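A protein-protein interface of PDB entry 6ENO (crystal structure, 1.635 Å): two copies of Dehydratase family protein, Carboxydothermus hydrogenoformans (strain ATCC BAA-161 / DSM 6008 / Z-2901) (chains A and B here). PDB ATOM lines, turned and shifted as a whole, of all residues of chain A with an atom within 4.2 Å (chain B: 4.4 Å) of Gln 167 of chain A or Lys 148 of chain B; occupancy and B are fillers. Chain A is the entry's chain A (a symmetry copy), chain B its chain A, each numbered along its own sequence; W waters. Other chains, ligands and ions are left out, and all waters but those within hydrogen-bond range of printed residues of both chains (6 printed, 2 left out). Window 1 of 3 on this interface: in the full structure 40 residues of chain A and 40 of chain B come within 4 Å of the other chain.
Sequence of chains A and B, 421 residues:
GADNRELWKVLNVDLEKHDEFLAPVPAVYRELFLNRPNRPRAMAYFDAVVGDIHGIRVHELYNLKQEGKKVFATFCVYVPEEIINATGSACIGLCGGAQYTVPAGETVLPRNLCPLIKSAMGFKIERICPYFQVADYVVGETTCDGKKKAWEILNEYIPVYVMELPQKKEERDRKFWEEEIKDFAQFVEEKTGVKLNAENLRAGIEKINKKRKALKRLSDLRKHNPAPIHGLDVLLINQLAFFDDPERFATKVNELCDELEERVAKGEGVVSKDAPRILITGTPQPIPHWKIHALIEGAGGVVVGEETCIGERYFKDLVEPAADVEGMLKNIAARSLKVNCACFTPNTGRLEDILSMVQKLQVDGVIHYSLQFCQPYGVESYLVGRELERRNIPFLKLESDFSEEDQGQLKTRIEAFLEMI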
ATOM      1  N   LEU A 165      14.246 -22.498  17.165  1.00  0.00           N
ATOM      2  CA  LEU A 165      13.324 -21.814  16.292  1.00  0.00           C
ATOM      3  C   LEU A 165      14.034 -21.531  14.983  1.00  0.00           C
ATOM      4  O   LEU A 165      15.183 -21.069  15.015  1.00  0.00           O
ATOM      5  CB  LEU A 165      12.880 -20.534  16.978  1.00  0.00           C
ATOM      6  CG  LEU A 165      11.732 -19.712  16.442  1.00  0.00           C
ATOM      7  CD1 LEU A 165      10.506 -20.547  16.392  1.00  0.00           C
ATOM      8  CD2 LEU A 165      11.496 -18.488  17.298  1.00  0.00           C
ATOM      9  N   PRO A 166      13.410 -21.801  13.833  1.00  0.00           N
ATOM     10  CA  PRO A 166      14.050 -21.466  12.543  1.00  0.00           C
ATOM     11  C   PRO A 166      14.067 -19.962  12.321  1.00  0.00           C
ATOM     12  O   PRO A 166      13.599 -19.206  13.169  1.00  0.00           O
ATOM     13  CB  PRO A 166      13.166 -22.186  11.521  1.00  0.00           C
ATOM     14  CG  PRO A 166      11.882 -22.362  12.137  1.00  0.00           C
ATOM     15  CD  PRO A 166      12.082 -22.419  13.616  1.00  0.00           C
ATOM     16  N   GLN A 167      14.632 -19.512  11.189  1.00  0.00           N
ATOM     17  CA  GLN A 167      14.794 -18.100  10.913  1.00  0.00           C
ATOM     18  C   GLN A 167      14.012 -17.615   9.705  1.00  0.00           C
ATOM     19  O   GLN A 167      14.052 -16.415   9.400  1.00  0.00           O
ATOM     20  CB  GLN A 167      16.290 -17.787  10.757  1.00  0.00           C
ATOM     21  CG  GLN A 167      17.034 -18.132  12.084  1.00  0.00           C
ATOM     22  CD  GLN A 167      18.499 -17.777  12.043  1.00  0.00           C
ATOM     23  OE1 GLN A 167      18.878 -16.659  12.345  1.00  0.00           O
ATOM     24  NE2 GLN A 167      19.318 -18.740  11.667  1.00  0.00           N
ATOM     25  N   LYS A 168      13.315 -18.500   9.003  1.00  0.00           N
ATOM     26  CA  LYS A 168      12.395 -18.140   7.934  1.00  0.00           C
ATOM     27  C   LYS A 168      11.087 -18.887   8.183  1.00  0.00           C
ATOM     28  O   LYS A 168      11.016 -19.726   9.087  1.00  0.00           O
ATOM     29  CB  LYS A 168      12.945 -18.524   6.539  1.00  0.00           C
ATOM     30  CG  LYS A 168      14.246 -17.815   6.163  1.00  0.00           C
ATOM     31  CD  LYS A 168      14.625 -18.112   4.699  1.00  0.00           C
ATOM     32  CE  LYS A 168      15.851 -17.350   4.255  1.00  0.00           C
ATOM     33  NZ  LYS A 168      16.142 -17.655   2.805  1.00  0.00           N
ATOM     34  N   CYS A 343      13.044 -11.626  14.597  1.00  0.00           N
ATOM     35  CA  CYS A 343      14.073 -12.653  14.390  1.00  0.00           C
ATOM     36  C   CYS A 343      13.839 -13.459  13.128  1.00  0.00           C
ATOM     37  O   CYS A 343      14.713 -14.237  12.735  1.00  0.00           O
ATOM     38  CB  CYS A 343      14.131 -13.588  15.610  1.00  0.00           C
ATOM     39  SG  CYS A 343      14.625 -12.662  17.124  1.00  0.00           S
ATOM     40  N   PHE A 344      12.688 -13.307  12.488  1.00  0.00           N
ATOM     41  CA  PHE A 344      12.435 -13.953  11.210  1.00  0.00           C
ATOM     42  C   PHE A 344      12.738 -12.999  10.080  1.00  0.00           C
ATOM     43  O   PHE A 344      12.627 -11.779  10.220  1.00  0.00           O
ATOM     44  CB  PHE A 344      10.999 -14.426  11.116  1.00  0.00           C
ATOM     45  CG  PHE A 344      10.717 -15.629  11.968  1.00  0.00           C
ATOM     46  CD1 PHE A 344      10.894 -16.897  11.460  1.00  0.00           C
ATOM     47  CD2 PHE A 344      10.321 -15.478  13.284  1.00  0.00           C
ATOM     48  CE1 PHE A 344      10.648 -17.998  12.219  1.00  0.00           C
ATOM     49  CE2 PHE A 344      10.119 -16.584  14.056  1.00  0.00           C
ATOM     50  CZ  PHE A 344      10.264 -17.849  13.516  1.00  0.00           C
ATOM     51  N   THR A 345      13.144 -13.580   8.958  1.00  0.00           N
ATOM     52  CA  THR A 345      13.373 -12.828   7.743  1.00  0.00           C
ATOM     53  C   THR A 345      12.663 -13.481   6.564  1.00  0.00           C
ATOM     54  O   THR A 345      12.670 -14.708   6.435  1.00  0.00           O
ATOM     55  CB  THR A 345      14.880 -12.702   7.460  1.00  0.00           C
ATOM     56  OG1 THR A 345      15.091 -11.803   6.382  1.00  0.00           O
ATOM     57  CG2 THR A 345      15.501 -14.036   7.111  1.00  0.00           C
ATOM     58  N   THR B 142      21.969 -16.314   7.297  1.00  0.00           N
ATOM     59  CA  THR B 142      21.319 -16.075   8.602  1.00  0.00           C
ATOM     60  C   THR B 142      22.254 -16.504   9.738  1.00  0.00           C
ATOM     61  O   THR B 142      22.062 -17.526  10.395  1.00  0.00           O
ATOM     62  CB  THR B 142      19.985 -16.815   8.699  1.00  0.00           C
ATOM     63  OG1 THR B 142      20.189 -18.216   8.529  1.00  0.00           O
ATOM     64  CG2 THR B 142      19.020 -16.288   7.635  1.00  0.00           C
ATOM     65  N   THR B 143      23.297 -15.694   9.938  1.00  0.00           N
ATOM     66  CA  THR B 143      24.204 -15.879  11.071  1.00  0.00           C
ATOM     67  C   THR B 143      23.820 -14.927  12.197  1.00  0.00           C
ATOM     68  O   THR B 143      22.881 -15.248  12.943  1.00  0.00           O
ATOM     69  CB  THR B 143      25.638 -15.671  10.656  1.00  0.00           C
ATOM     70  OG1 THR B 143      25.679 -14.500   9.850  1.00  0.00           O
ATOM     71  CG2 THR B 143      26.162 -16.847   9.864  1.00  0.00           C
ATOM     72  N   CYS B 144      24.483 -13.768  12.311  1.00  0.00           N
ATOM     73  CA  CYS B 144      24.195 -12.863  13.419  1.00  0.00           C
ATOM     74  C   CYS B 144      22.981 -12.007  13.107  1.00  0.00           C
ATOM     75  O   CYS B 144      22.554 -11.890  11.961  1.00  0.00           O
ATOM     76  CB  CYS B 144      25.367 -11.954  13.716  1.00  0.00           C
ATOM     77  SG  CYS B 144      25.824 -10.929  12.299  1.00  0.00           S
ATOM     78  N   ASP B 145      22.422 -11.400  14.160  1.00  0.00           N
ATOM     79  CA  ASP B 145      21.206 -10.622  14.011  1.00  0.00           C
ATOM     80  C   ASP B 145      21.409  -9.473  13.040  1.00  0.00           C
ATOM     81  O   ASP B 145      20.537  -9.190  12.215  1.00  0.00           O
ATOM     82  CB  ASP B 145      20.761 -10.063  15.366  1.00  0.00           C
ATOM     83  CG  ASP B 145      20.333 -11.150  16.356  1.00  0.00           C
ATOM     84  OD1 ASP B 145      19.933 -12.245  15.916  1.00  0.00           O
ATOM     85  OD2 ASP B 145      20.346 -10.864  17.577  1.00  0.00           O
ATOM     86  N   GLY B 146      22.532  -8.751  13.173  1.00  0.00           N
ATOM     87  CA  GLY B 146      22.753  -7.588  12.338  1.00  0.00           C
ATOM     88  C   GLY B 146      22.864  -7.941  10.864  1.00  0.00           C
ATOM     89  O   GLY B 146      22.335  -7.237  10.014  1.00  0.00           O
ATOM     90  N   LYS B 147      23.562  -9.019  10.536  1.00  0.00           N
ATOM     91  CA  LYS B 147      23.660  -9.393   9.123  1.00  0.00           C
ATOM     92  C   LYS B 147      22.303  -9.794   8.596  1.00  0.00           C
ATOM     93  O   LYS B 147      21.877  -9.343   7.534  1.00  0.00           O
ATOM     94  CB  LYS B 147      24.638 -10.541   8.915  1.00  0.00           C
ATOM     95  CG  LYS B 147      26.104 -10.110   8.777  1.00  0.00           C
ATOM     96  CD  LYS B 147      27.000 -11.343   8.917  1.00  0.00           C
ATOM     97  CE  LYS B 147      28.221 -11.262   8.026  1.00  0.00           C
ATOM     98  NZ  LYS B 147      28.956 -12.542   8.041  1.00  0.00           N
ATOM     99  N   LYS B 148      21.623 -10.670   9.329  1.00  0.00           N
ATOM    100  CA  LYS B 148      20.329 -11.177   8.883  1.00  0.00           C
ATOM    101  C   LYS B 148      19.376 -10.041   8.549  1.00  0.00           C
ATOM    102  O   LYS B 148      18.725 -10.050   7.511  1.00  0.00           O
ATOM    103  CB  LYS B 148      19.734 -12.064   9.971  1.00  0.00           C
ATOM    104  CG  LYS B 148      18.349 -12.561   9.648  1.00  0.00           C
ATOM    105  CD  LYS B 148      17.937 -13.667  10.611  1.00  0.00           C
ATOM    106  CE  LYS B 148      17.817 -13.171  12.079  1.00  0.00           C
ATOM    107  NZ  LYS B 148      17.337 -14.299  12.950  1.00  0.00           N
ATOM    108  N   LYS B 149      19.279  -9.043   9.415  1.00  0.00           N
ATOM    109  CA  LYS B 149      18.298  -8.000   9.157  1.00  0.00           C
ATOM    110  C   LYS B 149      18.834  -6.965   8.167  1.00  0.00           C
ATOM    111  O   LYS B 149      18.040  -6.317   7.481  1.00  0.00           O
ATOM    112  CB  LYS B 149      17.871  -7.340  10.488  1.00  0.00           C
ATOM    113  CG  LYS B 149      17.313  -8.361  11.520  1.00  0.00           C
ATOM    114  CD  LYS B 149      16.084  -9.127  10.963  1.00  0.00           C
ATOM    115  CE  LYS B 149      14.847  -8.251  10.852  1.00  0.00           C
ATOM    116  NZ  LYS B 149      13.674  -9.032  10.299  1.00  0.00           N
ATOM    117  N   ALA B 150      20.152  -6.837   8.049  1.00  0.00           N
ATOM    118  CA  ALA B 150      20.717  -5.884   7.093  1.00  0.00           C
ATOM    119  C   ALA B 150      20.464  -6.313   5.648  1.00  0.00           C
ATOM    120  O   ALA B 150      20.248  -5.449   4.788  1.00  0.00           O
ATOM    121  CB  ALA B 150      22.207  -5.717   7.344  1.00  0.00           C
ATOM    122  N   TRP B 151      20.448  -7.624   5.370  1.00  0.00           N
ATOM    123  CA  TRP B 151      20.194  -8.091   4.002  1.00  0.00           C
ATOM    124  C   TRP B 151      18.853  -7.581   3.477  1.00  0.00           C
ATOM    125  O   TRP B 151      18.704  -7.337   2.270  1.00  0.00           O
ATOM    126  CB  TRP B 151      20.225  -9.627   3.907  1.00  0.00           C
ATOM    127  CG  TRP B 151      21.408 -10.339   4.503  1.00  0.00           C
ATOM    128  CD1 TRP B 151      21.372 -11.497   5.259  1.00  0.00           C
ATOM    129  CD2 TRP B 151      22.801  -9.985   4.401  1.00  0.00           C
ATOM    130  NE1 TRP B 151      22.646 -11.854   5.632  1.00  0.00           N
ATOM    131  CE2 TRP B 151      23.537 -10.957   5.110  1.00  0.00           C
ATOM    132  CE3 TRP B 151      23.498  -8.944   3.774  1.00  0.00           C
ATOM    133  CZ2 TRP B 151      24.925 -10.912   5.222  1.00  0.00           C
ATOM    134  CZ3 TRP B 151      24.871  -8.912   3.885  1.00  0.00           C
ATOM    135  CH2 TRP B 151      25.568  -9.875   4.614  1.00  0.00           C
ATOM    136  N   GLU B 152      17.852  -7.472   4.351  1.00  0.00           N
ATOM    137  CA  GLU B 152      16.533  -7.011   3.919  1.00  0.00           C
ATOM    138  C   GLU B 152      16.612  -5.609   3.349  1.00  0.00           C
ATOM    139  O   GLU B 152      15.835  -5.250   2.460  1.00  0.00           O
ATOM    140  CB  GLU B 152      15.548  -7.060   5.089  1.00  0.00           C
ATOM    141  CG  GLU B 152      15.398  -8.437   5.770  1.00  0.00           C
ATOM    142  CD  GLU B 152      14.514  -8.412   6.984  1.00  0.00           C
ATOM    143  OE1 GLU B 152      14.001  -7.320   7.384  1.00  0.00           O
ATOM    144  OE2 GLU B 152      14.332  -9.495   7.536  1.00  0.00           O
ATOM    145  N   GLU B 164      19.823 -19.913   4.559  1.00  0.00           N
ATOM    146  CA  GLU B 164      19.463 -20.117   5.962  1.00  0.00           C
ATOM    147  C   GLU B 164      20.389 -21.154   6.585  1.00  0.00           C
ATOM    148  O   GLU B 164      20.230 -22.364   6.383  1.00  0.00           O
ATOM    149  CB  GLU B 164      17.998 -20.517   6.128  1.00  0.00           C
ATOM    150  CG  GLU B 164      17.649 -20.650   7.624  1.00  0.00           C
ATOM    151  CD  GLU B 164      16.208 -20.913   7.946  1.00  0.00           C
ATOM    152  OE1 GLU B 164      15.381 -21.068   7.027  1.00  0.00           O
ATOM    153  OE2 GLU B 164      15.911 -20.995   9.175  1.00  0.00           O
ATOM    154  N   LEU B 165      21.292 -20.676   7.382  1.00  0.00           N
ATOM    155  CA  LEU B 165      22.149 -21.519   8.178  1.00  0.00           C
ATOM    156  C   LEU B 165      21.407 -21.881   9.450  1.00  0.00           C
ATOM    157  O   LEU B 165      20.810 -20.989  10.067  1.00  0.00           O
ATOM    158  CB  LEU B 165      23.427 -20.754   8.474  1.00  0.00           C
ATOM    159  CG  LEU B 165      24.632 -21.437   9.077  1.00  0.00           C
ATOM    160  CD1 LEU B 165      25.064 -22.548   8.193  1.00  0.00           C
ATOM    161  CD2 LEU B 165      25.766 -20.457   9.278  1.00  0.00           C
ATOM    162  N   GLN B 167      21.068 -23.266  13.548  1.00  0.00           N
ATOM    163  CA  GLN B 167      21.691 -22.750  14.748  1.00  0.00           C
ATOM    164  C   GLN B 167      22.232 -23.828  15.672  1.00  0.00           C
ATOM    165  O   GLN B 167      22.817 -23.495  16.713  1.00  0.00           O
ATOM    166  CB  GLN B 167      20.690 -21.850  15.487  1.00  0.00           C
ATOM    167  CG  GLN B 167      20.293 -20.652  14.569  1.00  0.00           C
ATOM    168  CD  GLN B 167      19.372 -19.672  15.251  1.00  0.00           C
ATOM    169  OE1 GLN B 167      19.820 -18.759  15.922  1.00  0.00           O
ATOM    170  NE2 GLN B 167      18.080 -19.868  15.070  1.00  0.00           N
HETATM  171  O   HOH W   1      17.695 -11.625   5.360  1.00  0.00           O
HETATM  172  O   HOH W   2      19.824 -16.545  14.692  1.00  0.00           O
HETATM  173  O   HOH W   3      17.622 -13.224  15.698  1.00  0.00           O
HETATM  174  O   HOH W   4      17.418 -16.468  15.180  1.00  0.00           O
HETATM  175  O   HOH W   5      17.484 -22.219  13.472  1.00  0.00           O
HETATM  176  O   HOH W   6      17.952 -21.203  10.956  1.00  0.00           O
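O of Thr 142 of chain B is in hydrogen-bond range of NE2 of Gln 167 of chain A (3.3 Å). The side-chain amino group of Lys 148 of chain B lies within hydrogen-bond range of the side-chain amide oxygen of Gln 167 of chain A, 2.9 Å away. The side-chain amino group (NZ) of Lys 148 of chain B is in hydrogen-bond range of the backbone carbonyl oxygen (O) of Cys 343 of chain A, 2.6 Å away. The backbone carbonyl oxygen (O) of Phe 344 of chain A is in hydrogen-bond range of the side-chain amino group (NZ) of Lys 149 of chain B (2.9 Å). OG1 of Thr 345 of chain A lies within hydrogen-bond range of OE2 of Glu 152 of chain B (2.7 Å). N of Gln 167 of chain A is in hydrogen-bond range of OE2 of Glu 164 of chain B. O of Leu 165 of chain B sits at hydrogen-bond distance from NE2 of Gln 167 of chain A. The side-chain amide nitrogen of Gln 167 of chain B is in hydrogen-bond range of the backbone carbonyl oxygen of Leu 165 of chain A, at 3.1 Å.
The side-chain hydroxyl (OG1) of Thr 142 of chain B sits at hydrogen-bond distance from the backbone NH (N) of Leu 165 of chain B (2.9 Å). NZ of Lys 149 of chain B is in salt-bridge range of OE2 of Glu 152 of chain B (2.9 Å). N of Thr 345 of chain A is in hydrogen-bond range of O of Gln 167 of chain A.
Glu 164 of chain B touches Pro 166 of chain A. Gln 167 of chain B touches Gln 167 of chain A (NE2 to CG, 3.6 Å). OE1 of Glu 164 of chain B touches CG of Lys 168 of chain A, 3.6 Å away. O of Phe 344 of chain A touches OE2 of Glu 152 of chain B, 3.9 Å away.
Printed residues of chain A within 4 Å of Lys 148 of chain B: Gln 167 and Cys 343. Printed residues of chain B within 4 Å of Pro 166 of chain A: Glu 164. Of the printed residues of chain B, Leu 165 of chain A touches Gln 167 (3.1 Å). Printed residues of chain A within 4 Å of Glu 164 of chain B: Pro 166 (3.8 Å), Gln 167 (2.8 Å) and Lys 168 (3.6 Å). The nearest residue of chain B that does not touch Gln 167 of chain A is Thr 143 of chain B (4.3 Å).
Of the 7 printed residues of chain A, 7 touch a printed residue of chain B. Along chain A the printed residues that touch a printed residue of chain B span positions 165 to 345. Among the printed residues, 12 pairs touch across the chains. Among the printed residues, no Asp or Glu carboxylate lies within 4 Å of a Lys or Arg side-chain nitrogen of the other chain.
Leu 165 of chain A touches Gln 167 of chain B, and with the chains exchanged Gln 167 of chain A touches Leu 165 of chain B. Gln 167 of chain B touches its own counterpart, Gln 167 of chain A. Positions printed for both chains: 165 and 167.
Water W3 lies within hydrogen-bond range of OD1 of Asp 145 of chain B, NZ of Lys 148 of chain B and SG of Cys 343 of chain A. Water W2 bridges OE1 of Gln 167 of chain A (2.5 Å) and OE1 of Gln 167 of chain B (2.5 Å). Water W6 lies within hydrogen-bond range of the side-chain carboxylate of Glu 164 of chain B (2.7 Å), the side-chain amide nitrogen of Gln 167 of chain A (2.9 Å) and the backbone carbonyl oxygen of Leu 165 of chain B (3.0 Å). Water W1 lies within hydrogen-bond range of OG1 of Thr 345 of chain A (2.8 Å) and O of Lys 148 of chain B (2.9 Å). Water W5 lies within hydrogen-bond range of NE2 of Gln 167 of chain B (2.9 Å) and O of Leu 165 of chain A (3.0 Å). Water W4 lies within hydrogen-bond range of the side-chain amino group (NZ) of Lys 148 of chain B (3.1 Å), the side-chain amide oxygen (OE1) of Gln 167 of chain A (3.2 Å) and the side-chain amide oxygen (OE1) of Gln 167 of chain B (3.4 Å).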
